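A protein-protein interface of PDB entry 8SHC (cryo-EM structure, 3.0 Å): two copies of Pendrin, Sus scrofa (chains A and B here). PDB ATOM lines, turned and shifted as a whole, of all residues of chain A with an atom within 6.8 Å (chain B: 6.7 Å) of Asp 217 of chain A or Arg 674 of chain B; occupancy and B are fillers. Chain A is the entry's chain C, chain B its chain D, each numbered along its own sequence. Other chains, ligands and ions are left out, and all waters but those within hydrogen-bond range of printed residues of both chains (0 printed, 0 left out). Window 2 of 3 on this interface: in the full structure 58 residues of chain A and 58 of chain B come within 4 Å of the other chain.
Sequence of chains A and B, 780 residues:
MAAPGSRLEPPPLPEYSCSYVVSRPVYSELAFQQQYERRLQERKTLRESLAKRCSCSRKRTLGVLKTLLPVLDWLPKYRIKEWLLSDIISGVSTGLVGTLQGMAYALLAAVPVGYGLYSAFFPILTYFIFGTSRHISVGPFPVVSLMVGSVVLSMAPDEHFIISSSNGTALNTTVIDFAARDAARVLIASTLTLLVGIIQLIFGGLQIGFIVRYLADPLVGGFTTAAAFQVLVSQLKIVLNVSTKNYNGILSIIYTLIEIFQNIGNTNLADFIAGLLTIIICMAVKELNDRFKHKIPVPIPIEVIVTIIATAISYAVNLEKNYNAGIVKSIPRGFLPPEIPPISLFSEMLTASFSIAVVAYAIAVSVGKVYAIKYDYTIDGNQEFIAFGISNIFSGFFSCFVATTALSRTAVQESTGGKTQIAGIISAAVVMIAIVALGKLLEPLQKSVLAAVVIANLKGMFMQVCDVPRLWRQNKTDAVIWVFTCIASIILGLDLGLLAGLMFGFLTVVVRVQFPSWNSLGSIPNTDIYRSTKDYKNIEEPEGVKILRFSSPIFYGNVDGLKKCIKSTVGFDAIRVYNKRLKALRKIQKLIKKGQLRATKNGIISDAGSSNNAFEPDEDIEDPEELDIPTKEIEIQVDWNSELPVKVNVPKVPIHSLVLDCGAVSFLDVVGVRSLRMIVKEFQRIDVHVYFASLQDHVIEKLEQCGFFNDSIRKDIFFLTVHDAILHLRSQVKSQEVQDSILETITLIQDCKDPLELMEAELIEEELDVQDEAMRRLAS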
ATOM      1  N   ARG A 213      26.190  19.811  15.853  1.00  0.00           N
ATOM      2  CA  ARG A 213      26.928  19.106  14.812  1.00  0.00           C
ATOM      3  C   ARG A 213      28.291  18.657  15.320  1.00  0.00           C
ATOM      4  O   ARG A 213      28.811  17.622  14.891  1.00  0.00           O
ATOM      5  CB  ARG A 213      27.083  19.993  13.578  1.00  0.00           C
ATOM      6  CG  ARG A 213      25.779  20.345  12.886  1.00  0.00           C
ATOM      7  CD  ARG A 213      25.978  21.492  11.913  1.00  0.00           C
ATOM      8  NE  ARG A 213      24.731  21.908  11.284  1.00  0.00           N
ATOM      9  CZ  ARG A 213      24.657  22.625  10.172  1.00  0.00           C
ATOM     10  NH1 ARG A 213      25.745  23.027   9.535  1.00  0.00           N
ATOM     11  NH2 ARG A 213      23.462  22.947   9.686  1.00  0.00           N
ATOM     12  N   TYR A 214      28.875  19.412  16.254  1.00  0.00           N
ATOM     13  CA  TYR A 214      30.198  19.085  16.771  1.00  0.00           C
ATOM     14  C   TYR A 214      30.204  17.847  17.657  1.00  0.00           C
ATOM     15  O   TYR A 214      31.286  17.349  17.985  1.00  0.00           O
ATOM     16  CB  TYR A 214      30.766  20.277  17.543  1.00  0.00           C
ATOM     17  CG  TYR A 214      31.036  21.486  16.677  1.00  0.00           C
ATOM     18  CD1 TYR A 214      31.800  21.379  15.522  1.00  0.00           C
ATOM     19  CD2 TYR A 214      30.527  22.734  17.011  1.00  0.00           C
ATOM     20  CE1 TYR A 214      32.051  22.478  14.727  1.00  0.00           C
ATOM     21  CE2 TYR A 214      30.773  23.840  16.221  1.00  0.00           C
ATOM     22  CZ  TYR A 214      31.535  23.707  15.080  1.00  0.00           C
ATOM     23  OH  TYR A 214      31.782  24.806  14.290  1.00  0.00           O
ATOM     24  N   LEU A 215      29.037  17.340  18.049  1.00  0.00           N
ATOM     25  CA  LEU A 215      28.942  16.125  18.856  1.00  0.00           C
ATOM     26  C   LEU A 215      28.924  14.925  17.917  1.00  0.00           C
ATOM     27  O   LEU A 215      27.870  14.474  17.466  1.00  0.00           O
ATOM     28  CB  LEU A 215      27.702  16.163  19.742  1.00  0.00           C
ATOM     29  CG  LEU A 215      27.647  17.260  20.806  1.00  0.00           C
ATOM     30  CD1 LEU A 215      26.453  17.057  21.720  1.00  0.00           C
ATOM     31  CD2 LEU A 215      28.931  17.289  21.614  1.00  0.00           C
ATOM     32  N   ALA A 216      30.110  14.401  17.620  1.00  0.00           N
ATOM     33  CA  ALA A 216      30.232  13.264  16.720  1.00  0.00           C
ATOM     34  C   ALA A 216      29.631  12.008  17.342  1.00  0.00           C
ATOM     35  O   ALA A 216      29.540  11.873  18.564  1.00  0.00           O
ATOM     36  CB  ALA A 216      31.697  13.021  16.362  1.00  0.00           C
ATOM     37  N   ASP A 217      29.203  11.088  16.478  1.00  0.00           N
ATOM     38  CA  ASP A 217      28.570   9.857  16.954  1.00  0.00           C
ATOM     39  C   ASP A 217      29.491   8.990  17.807  1.00  0.00           C
ATOM     40  O   ASP A 217      29.037   8.505  18.858  1.00  0.00           O
ATOM     41  CB  ASP A 217      28.012   9.074  15.759  1.00  0.00           C
ATOM     42  CG  ASP A 217      27.106   7.934  16.182  1.00  0.00           C
ATOM     43  OD1 ASP A 217      26.665   7.922  17.350  1.00  0.00           O
ATOM     44  OD2 ASP A 217      26.838   7.046  15.347  1.00  0.00           O
ATOM     45  N   PRO A 218      30.748   8.716  17.422  1.00  0.00           N
ATOM     46  CA  PRO A 218      31.599   7.899  18.307  1.00  0.00           C
ATOM     47  C   PRO A 218      31.793   8.494  19.692  1.00  0.00           C
ATOM     48  O   PRO A 218      31.782   7.755  20.687  1.00  0.00           O
ATOM     49  CB  PRO A 218      32.920   7.815  17.532  1.00  0.00           C
ATOM     50  CG  PRO A 218      32.519   7.959  16.113  1.00  0.00           C
ATOM     51  CD  PRO A 218      31.413   8.971  16.130  1.00  0.00           C
ATOM     52  N   LEU A 219      31.955   9.816  19.795  1.00  0.00           N
ATOM     53  CA  LEU A 219      32.117  10.407  21.117  1.00  0.00           C
ATOM     54  C   LEU A 219      30.815  10.363  21.902  1.00  0.00           C
ATOM     55  O   LEU A 219      30.840  10.212  23.126  1.00  0.00           O
ATOM     56  CB  LEU A 219      32.653  11.840  21.012  1.00  0.00           C
ATOM     57  CG  LEU A 219      31.852  12.993  20.405  1.00  0.00           C
ATOM     58  CD1 LEU A 219      30.933  13.651  21.429  1.00  0.00           C
ATOM     59  CD2 LEU A 219      32.796  14.023  19.806  1.00  0.00           C
ATOM     60  N   VAL A 220      29.673  10.462  21.217  1.00  0.00           N
ATOM     61  CA  VAL A 220      28.389  10.288  21.890  1.00  0.00           C
ATOM     62  C   VAL A 220      28.275   8.880  22.459  1.00  0.00           C
ATOM     63  O   VAL A 220      27.842   8.691  23.601  1.00  0.00           O
ATOM     64  CB  VAL A 220      27.228  10.610  20.931  1.00  0.00           C
ATOM     65  CG1 VAL A 220      25.916  10.085  21.489  1.00  0.00           C
ATOM     66  CG2 VAL A 220      27.137  12.107  20.698  1.00  0.00           C
ATOM     67  N   GLY A 221      28.670   7.871  21.679  1.00  0.00           N
ATOM     68  CA  GLY A 221      28.614   6.502  22.172  1.00  0.00           C
ATOM     69  C   GLY A 221      29.538   6.261  23.351  1.00  0.00           C
ATOM     70  O   GLY A 221      29.157   5.615  24.334  1.00  0.00           O
ATOM     71  N   GLY A 222      30.766   6.778  23.273  1.00  0.00           N
ATOM     72  CA  GLY A 222      31.688   6.634  24.391  1.00  0.00           C
ATOM     73  C   GLY A 222      31.199   7.337  25.644  1.00  0.00           C
ATOM     74  O   GLY A 222      31.273   6.787  26.749  1.00  0.00           O
ATOM     75  N   ARG A 470      33.612  -3.136  14.951  1.00  0.00           N
ATOM     76  CA  ARG A 470      33.310  -2.852  13.551  1.00  0.00           C
ATOM     77  C   ARG A 470      33.705  -1.427  13.190  1.00  0.00           C
ATOM     78  O   ARG A 470      34.198  -1.169  12.084  1.00  0.00           O
ATOM     79  CB  ARG A 470      31.828  -3.096  13.271  1.00  0.00           C
ATOM     80  CG  ARG A 470      31.369  -2.646  11.892  1.00  0.00           C
ATOM     81  CD  ARG A 470      29.940  -2.126  11.914  1.00  0.00           C
ATOM     82  NE  ARG A 470      29.695  -1.217  13.026  1.00  0.00           N
ATOM     83  CZ  ARG A 470      29.655   0.103  12.918  1.00  0.00           C
ATOM     84  NH1 ARG A 470      29.850   0.709  11.758  1.00  0.00           N
ATOM     85  NH2 ARG A 470      29.413   0.836  14.002  1.00  0.00           N
ATOM     86  N   LEU A 471      33.499  -0.488  14.116  1.00  0.00           N
ATOM     87  CA  LEU A 471      33.932   0.886  13.896  1.00  0.00           C
ATOM     88  C   LEU A 471      35.438   0.957  13.680  1.00  0.00           C
ATOM     89  O   LEU A 471      35.912   1.688  12.803  1.00  0.00           O
ATOM     90  CB  LEU A 471      33.518   1.756  15.082  1.00  0.00           C
ATOM     91  CG  LEU A 471      33.569   3.272  14.895  1.00  0.00           C
ATOM     92  CD1 LEU A 471      32.531   3.722  13.881  1.00  0.00           C
ATOM     93  CD2 LEU A 471      33.364   3.973  16.227  1.00  0.00           C
ATOM     94  N   GLN A 474      36.260  -0.344  10.184  1.00  0.00           N
ATOM     95  CA  GLN A 474      35.884   0.526   9.075  1.00  0.00           C
ATOM     96  C   GLN A 474      36.756   1.777   8.992  1.00  0.00           C
ATOM     97  O   GLN A 474      37.323   2.072   7.936  1.00  0.00           O
ATOM     98  CB  GLN A 474      34.410   0.922   9.195  1.00  0.00           C
ATOM     99  CG  GLN A 474      33.439  -0.187   8.838  1.00  0.00           C
ATOM    100  CD  GLN A 474      31.997   0.212   9.064  1.00  0.00           C
ATOM    101  OE1 GLN A 474      31.706   1.104   9.860  1.00  0.00           O
ATOM    102  NE2 GLN A 474      31.083  -0.450   8.366  1.00  0.00           N
ATOM    103  N   ASP A 478      37.543   7.039  13.900  1.00  0.00           N
ATOM    104  CA  ASP A 478      36.301   7.022  14.667  1.00  0.00           C
ATOM    105  C   ASP A 478      36.427   6.150  15.911  1.00  0.00           C
ATOM    106  O   ASP A 478      35.942   6.521  16.986  1.00  0.00           O
ATOM    107  CB  ASP A 478      35.149   6.547  13.785  1.00  0.00           C
ATOM    108  CG  ASP A 478      34.818   7.534  12.682  1.00  0.00           C
ATOM    109  OD1 ASP A 478      34.223   8.589  12.987  1.00  0.00           O
ATOM    110  OD2 ASP A 478      35.158   7.260  11.514  1.00  0.00           O
ATOM    111  N   ILE A 481      38.454   8.051  18.447  1.00  0.00           N
ATOM    112  CA  ILE A 481      37.626   9.061  19.105  1.00  0.00           C
ATOM    113  C   ILE A 481      36.714   8.414  20.140  1.00  0.00           C
ATOM    114  O   ILE A 481      36.566   8.918  21.261  1.00  0.00           O
ATOM    115  CB  ILE A 481      36.824   9.859  18.061  1.00  0.00           C
ATOM    116  CG1 ILE A 481      37.752  10.761  17.247  1.00  0.00           C
ATOM    117  CG2 ILE A 481      35.738  10.686  18.733  1.00  0.00           C
ATOM    118  CD1 ILE A 481      37.080  11.417  16.061  1.00  0.00           C
ATOM    119  N   TRP A 482      36.091   7.289  19.781  1.00  0.00           N
ATOM    120  CA  TRP A 482      35.230   6.560  20.712  1.00  0.00           C
ATOM    121  C   TRP A 482      35.984   6.184  21.982  1.00  0.00           C
ATOM    122  O   TRP A 482      35.533   6.471  23.100  1.00  0.00           O
ATOM    123  CB  TRP A 482      34.685   5.308  20.017  1.00  0.00           C
ATOM    124  CG  TRP A 482      33.421   4.737  20.595  1.00  0.00           C
ATOM    125  CD1 TRP A 482      32.170   4.819  20.060  1.00  0.00           C
ATOM    126  CD2 TRP A 482      33.293   3.962  21.795  1.00  0.00           C
ATOM    127  NE1 TRP A 482      31.268   4.163  20.859  1.00  0.00           N
ATOM    128  CE2 TRP A 482      31.932   3.627  21.930  1.00  0.00           C
ATOM    129  CE3 TRP A 482      34.194   3.527  22.771  1.00  0.00           C
ATOM    130  CZ2 TRP A 482      31.450   2.879  23.003  1.00  0.00           C
ATOM    131  CZ3 TRP A 482      33.714   2.784  23.835  1.00  0.00           C
ATOM    132  CH2 TRP A 482      32.356   2.468  23.941  1.00  0.00           C
ATOM    133  N   TYR B 556      30.728  15.259   9.402  1.00  0.00           N
ATOM    134  CA  TYR B 556      29.394  15.476   9.965  1.00  0.00           C
ATOM    135  C   TYR B 556      28.878  16.899   9.739  1.00  0.00           C
ATOM    136  O   TYR B 556      27.773  17.096   9.213  1.00  0.00           O
ATOM    137  CB  TYR B 556      29.397  15.107  11.451  1.00  0.00           C
ATOM    138  CG  TYR B 556      30.621  15.553  12.228  1.00  0.00           C
ATOM    139  CD1 TYR B 556      30.714  16.832  12.757  1.00  0.00           C
ATOM    140  CD2 TYR B 556      31.683  14.681  12.437  1.00  0.00           C
ATOM    141  CE1 TYR B 556      31.831  17.232  13.469  1.00  0.00           C
ATOM    142  CE2 TYR B 556      32.802  15.072  13.148  1.00  0.00           C
ATOM    143  CZ  TYR B 556      32.871  16.348  13.662  1.00  0.00           C
ATOM    144  OH  TYR B 556      33.983  16.745  14.369  1.00  0.00           O
ATOM    145  N   LYS B 563      23.638  18.294   2.782  1.00  0.00           N
ATOM    146  CA  LYS B 563      22.205  18.046   2.674  1.00  0.00           C
ATOM    147  C   LYS B 563      21.445  19.345   2.439  1.00  0.00           C
ATOM    148  O   LYS B 563      20.556  19.408   1.578  1.00  0.00           O
ATOM    149  CB  LYS B 563      21.691  17.338   3.927  1.00  0.00           C
ATOM    150  CG  LYS B 563      22.202  15.917   4.097  1.00  0.00           C
ATOM    151  CD  LYS B 563      21.629  15.269   5.346  1.00  0.00           C
ATOM    152  CE  LYS B 563      22.157  13.856   5.530  1.00  0.00           C
ATOM    153  NZ  LYS B 563      21.612  13.211   6.757  1.00  0.00           N
ATOM    154  N   ASP B 669      34.664   9.973   6.185  1.00  0.00           N
ATOM    155  CA  ASP B 669      34.441   9.233   7.421  1.00  0.00           C
ATOM    156  C   ASP B 669      33.164   8.403   7.297  1.00  0.00           C
ATOM    157  O   ASP B 669      32.504   8.388   6.256  1.00  0.00           O
ATOM    158  CB  ASP B 669      34.379  10.182   8.621  1.00  0.00           C
ATOM    159  CG  ASP B 669      33.256  11.192   8.516  1.00  0.00           C
ATOM    160  OD1 ASP B 669      32.680  11.339   7.417  1.00  0.00           O
ATOM    161  OD2 ASP B 669      32.946  11.844   9.534  1.00  0.00           O
ATOM    162  N   VAL B 670      32.817   7.705   8.382  1.00  0.00           N
ATOM    163  CA  VAL B 670      31.662   6.810   8.351  1.00  0.00           C
ATOM    164  C   VAL B 670      30.362   7.602   8.239  1.00  0.00           C
ATOM    165  O   VAL B 670      29.417   7.174   7.562  1.00  0.00           O
ATOM    166  CB  VAL B 670      31.666   5.883   9.581  1.00  0.00           C
ATOM    167  CG1 VAL B 670      32.855   4.940   9.524  1.00  0.00           C
ATOM    168  CG2 VAL B 670      31.700   6.691  10.869  1.00  0.00           C
ATOM    169  N   VAL B 671      30.289   8.761   8.897  1.00  0.00           N
ATOM    170  CA  VAL B 671      29.085   9.585   8.823  1.00  0.00           C
ATOM    171  C   VAL B 671      28.865  10.077   7.399  1.00  0.00           C
ATOM    172  O   VAL B 671      27.730  10.119   6.908  1.00  0.00           O
ATOM    173  CB  VAL B 671      29.174  10.752   9.824  1.00  0.00           C
ATOM    174  CG1 VAL B 671      27.905  11.588   9.783  1.00  0.00           C
ATOM    175  CG2 VAL B 671      29.428  10.226  11.228  1.00  0.00           C
ATOM    176  N   GLY B 672      29.946  10.454   6.711  1.00  0.00           N
ATOM    177  CA  GLY B 672      29.820  10.866   5.323  1.00  0.00           C
ATOM    178  C   GLY B 672      29.320   9.752   4.423  1.00  0.00           C
ATOM    179  O   GLY B 672      28.476   9.976   3.553  1.00  0.00           O
ATOM    180  N   VAL B 673      29.829   8.534   4.626  1.00  0.00           N
ATOM    181  CA  VAL B 673      29.375   7.396   3.831  1.00  0.00           C
ATOM    182  C   VAL B 673      27.901   7.117   4.094  1.00  0.00           C
ATOM    183  O   VAL B 673      27.128   6.848   3.165  1.00  0.00           O
ATOM    184  CB  VAL B 673      30.246   6.159   4.119  1.00  0.00           C
ATOM    185  CG1 VAL B 673      29.764   4.968   3.306  1.00  0.00           C
ATOM    186  CG2 VAL B 673      31.705   6.455   3.819  1.00  0.00           C
ATOM    187  N   ARG B 674      27.488   7.170   5.364  1.00  0.00           N
ATOM    188  CA  ARG B 674      26.083   6.956   5.694  1.00  0.00           C
ATOM    189  C   ARG B 674      25.197   8.011   5.045  1.00  0.00           C
ATOM    190  O   ARG B 674      24.131   7.691   4.502  1.00  0.00           O
ATOM    191  CB  ARG B 674      25.893   6.963   7.211  1.00  0.00           C
ATOM    192  CG  ARG B 674      26.437   5.737   7.921  1.00  0.00           C
ATOM    193  CD  ARG B 674      26.432   5.935   9.428  1.00  0.00           C
ATOM    194  NE  ARG B 674      27.248   4.943  10.118  1.00  0.00           N
ATOM    195  CZ  ARG B 674      27.785   5.120  11.318  1.00  0.00           C
ATOM    196  NH1 ARG B 674      27.615   6.244  11.993  1.00  0.00           N
ATOM    197  NH2 ARG B 674      28.511   4.143  11.854  1.00  0.00           N
ATOM    198  N   SER B 675      25.621   9.276   5.092  1.00  0.00           N
ATOM    199  CA  SER B 675      24.840  10.345   4.478  1.00  0.00           C
ATOM    200  C   SER B 675      24.736  10.157   2.969  1.00  0.00           C
ATOM    201  O   SER B 675      23.664  10.357   2.387  1.00  0.00           O
ATOM    202  CB  SER B 675      25.457  11.702   4.809  1.00  0.00           C
ATOM    203  OG  SER B 675      25.542  11.890   6.210  1.00  0.00           O
ATOM    204  N   LEU B 676      25.840   9.781   2.318  1.00  0.00           N
ATOM    205  CA  LEU B 676      25.800   9.546   0.877  1.00  0.00           C
ATOM    206  C   LEU B 676      24.870   8.391   0.530  1.00  0.00           C
ATOM    207  O   LEU B 676      24.093   8.476  -0.431  1.00  0.00           O
ATOM    208  CB  LEU B 676      27.209   9.279   0.347  1.00  0.00           C
ATOM    209  CG  LEU B 676      28.196  10.446   0.392  1.00  0.00           C
ATOM    210  CD1 LEU B 676      29.533  10.037  -0.202  1.00  0.00           C
ATOM    211  CD2 LEU B 676      27.631  11.656  -0.335  1.00  0.00           C
ATOM    212  N   ARG B 677      24.932   7.302   1.300  1.00  0.00           N
ATOM    213  CA  ARG B 677      24.046   6.167   1.056  1.00  0.00           C
ATOM    214  C   ARG B 677      22.585   6.572   1.210  1.00  0.00           C
ATOM    215  O   ARG B 677      21.736   6.216   0.382  1.00  0.00           O
ATOM    216  CB  ARG B 677      24.390   5.024   2.010  1.00  0.00           C
ATOM    217  CG  ARG B 677      24.337   3.643   1.382  1.00  0.00           C
ATOM    218  CD  ARG B 677      24.356   2.564   2.450  1.00  0.00           C
ATOM    219  NE  ARG B 677      25.643   2.501   3.134  1.00  0.00           N
ATOM    220  CZ  ARG B 677      25.798   2.571   4.448  1.00  0.00           C
ATOM    221  NH1 ARG B 677      24.761   2.713   5.259  1.00  0.00           N
ATOM    222  NH2 ARG B 677      27.022   2.501   4.963  1.00  0.00           N
ATOM    223  N   MET B 678      22.277   7.329   2.268  1.00  0.00           N
ATOM    224  CA  MET B 678      20.906   7.780   2.480  1.00  0.00           C
ATOM    225  C   MET B 678      20.440   8.683   1.346  1.00  0.00           C
ATOM    226  O   MET B 678      19.302   8.567   0.881  1.00  0.00           O
ATOM    227  CB  MET B 678      20.792   8.500   3.823  1.00  0.00           C
ATOM    228  CG  MET B 678      20.943   7.589   5.028  1.00  0.00           C
ATOM    229  SD  MET B 678      20.849   8.483   6.591  1.00  0.00           S
ATOM    230  CE  MET B 678      19.363   9.451   6.339  1.00  0.00           C
ATOM    231  N   ILE B 679      21.306   9.590   0.886  1.00  0.00           N
ATOM    232  CA  ILE B 679      20.939  10.488  -0.206  1.00  0.00           C
ATOM    233  C   ILE B 679      20.637   9.689  -1.469  1.00  0.00           C
ATOM    234  O   ILE B 679      19.629   9.923  -2.149  1.00  0.00           O
ATOM    235  CB  ILE B 679      22.052  11.524  -0.446  1.00  0.00           C
ATOM    236  CG1 ILE B 679      22.062  12.566   0.674  1.00  0.00           C
ATOM    237  CG2 ILE B 679      21.883  12.196  -1.801  1.00  0.00           C
ATOM    238  CD1 ILE B 679      23.283  13.459   0.665  1.00  0.00           C
ATOM    239  N   PHE B 708      29.826   0.732   1.476  1.00  0.00           N
ATOM    240  CA  PHE B 708      28.969   1.532   0.606  1.00  0.00           C
ATOM    241  C   PHE B 708      28.365   0.690  -0.511  1.00  0.00           C
ATOM    242  O   PHE B 708      27.177   0.826  -0.824  1.00  0.00           O
ATOM    243  CB  PHE B 708      29.764   2.700   0.024  1.00  0.00           C
ATOM    244  CG  PHE B 708      28.929   3.676  -0.754  1.00  0.00           C
ATOM    245  CD1 PHE B 708      28.240   4.689  -0.108  1.00  0.00           C
ATOM    246  CD2 PHE B 708      28.837   3.586  -2.133  1.00  0.00           C
ATOM    247  CE1 PHE B 708      27.473   5.588  -0.821  1.00  0.00           C
ATOM    248  CE2 PHE B 708      28.070   4.482  -2.851  1.00  0.00           C
ATOM    249  CZ  PHE B 708      27.388   5.485  -2.195  1.00  0.00           C
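The guanidinium group (NH1) of Arg 674 of chain B lies within salt-bridge range of the side-chain carboxylate (OD2) of Asp 217 of chain A.
Printed residues of chain B within 4 Å of Arg 213 of chain A: Tyr 556 (3.0 Å).
Of the printed residues of chain B, Ala 216 of chain A touches Tyr 556.
Asp 217 of chain A touches just one residue of chain B: Arg 674.
Leu 219 of chain A touches none of the printed residues of chain B.
Printed residues of chain B within 4 Å of Asp 478 of chain A: Val 670.
Of the printed residues of chain A, Val 670 of chain B touches Asp 478 (3.6 Å).
Arg 674 of chain B touches just these residues of chain A: Asp 217 (3.5 Å) and Arg 470 (3.7 Å).
The nearest residue of chain B that does not touch Asp 217 of chain A is Val 671 of chain B (4.9 Å).
The nearest printed residue of chain A that does not touch Tyr 556 of chain B is Tyr 214 of chain A (4.1 Å).
Of the 16 printed residues of chain A, 5 touch a printed residue of chain B.
Hydrophobic or aromatic side chains of chain A that line the printed part of chain B: Ala 216.
Of the 14 printed residues of chain B, 3 touch a printed residue of chain A.
Hydrophobic or aromatic side chains of chain B within 4 Å of the printed part of chain A: Tyr 556 and Val 670.
Among the printed residues, 5 pairs touch across the chains.
NH1 of Arg 470 of chain A sits at hydrogen-bond distance from OE1 of Gln 474 of chain A (2.7 Å).
No position is printed for both chains.
CD1 of Tyr 556 of chain B touches O of Arg 213 of chain A, 3.0 Å away.
CB of Ala 216 of chain A touches CE2 of Tyr 556 of chain B (3.97 Å).
Arg 470 of chain A touches Arg 674 of chain B (NH1 to NH2, 3.7 Å).
Asp 478 of chain A touches Val 670 of chain B (OD2 to CG2, 3.6 Å).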
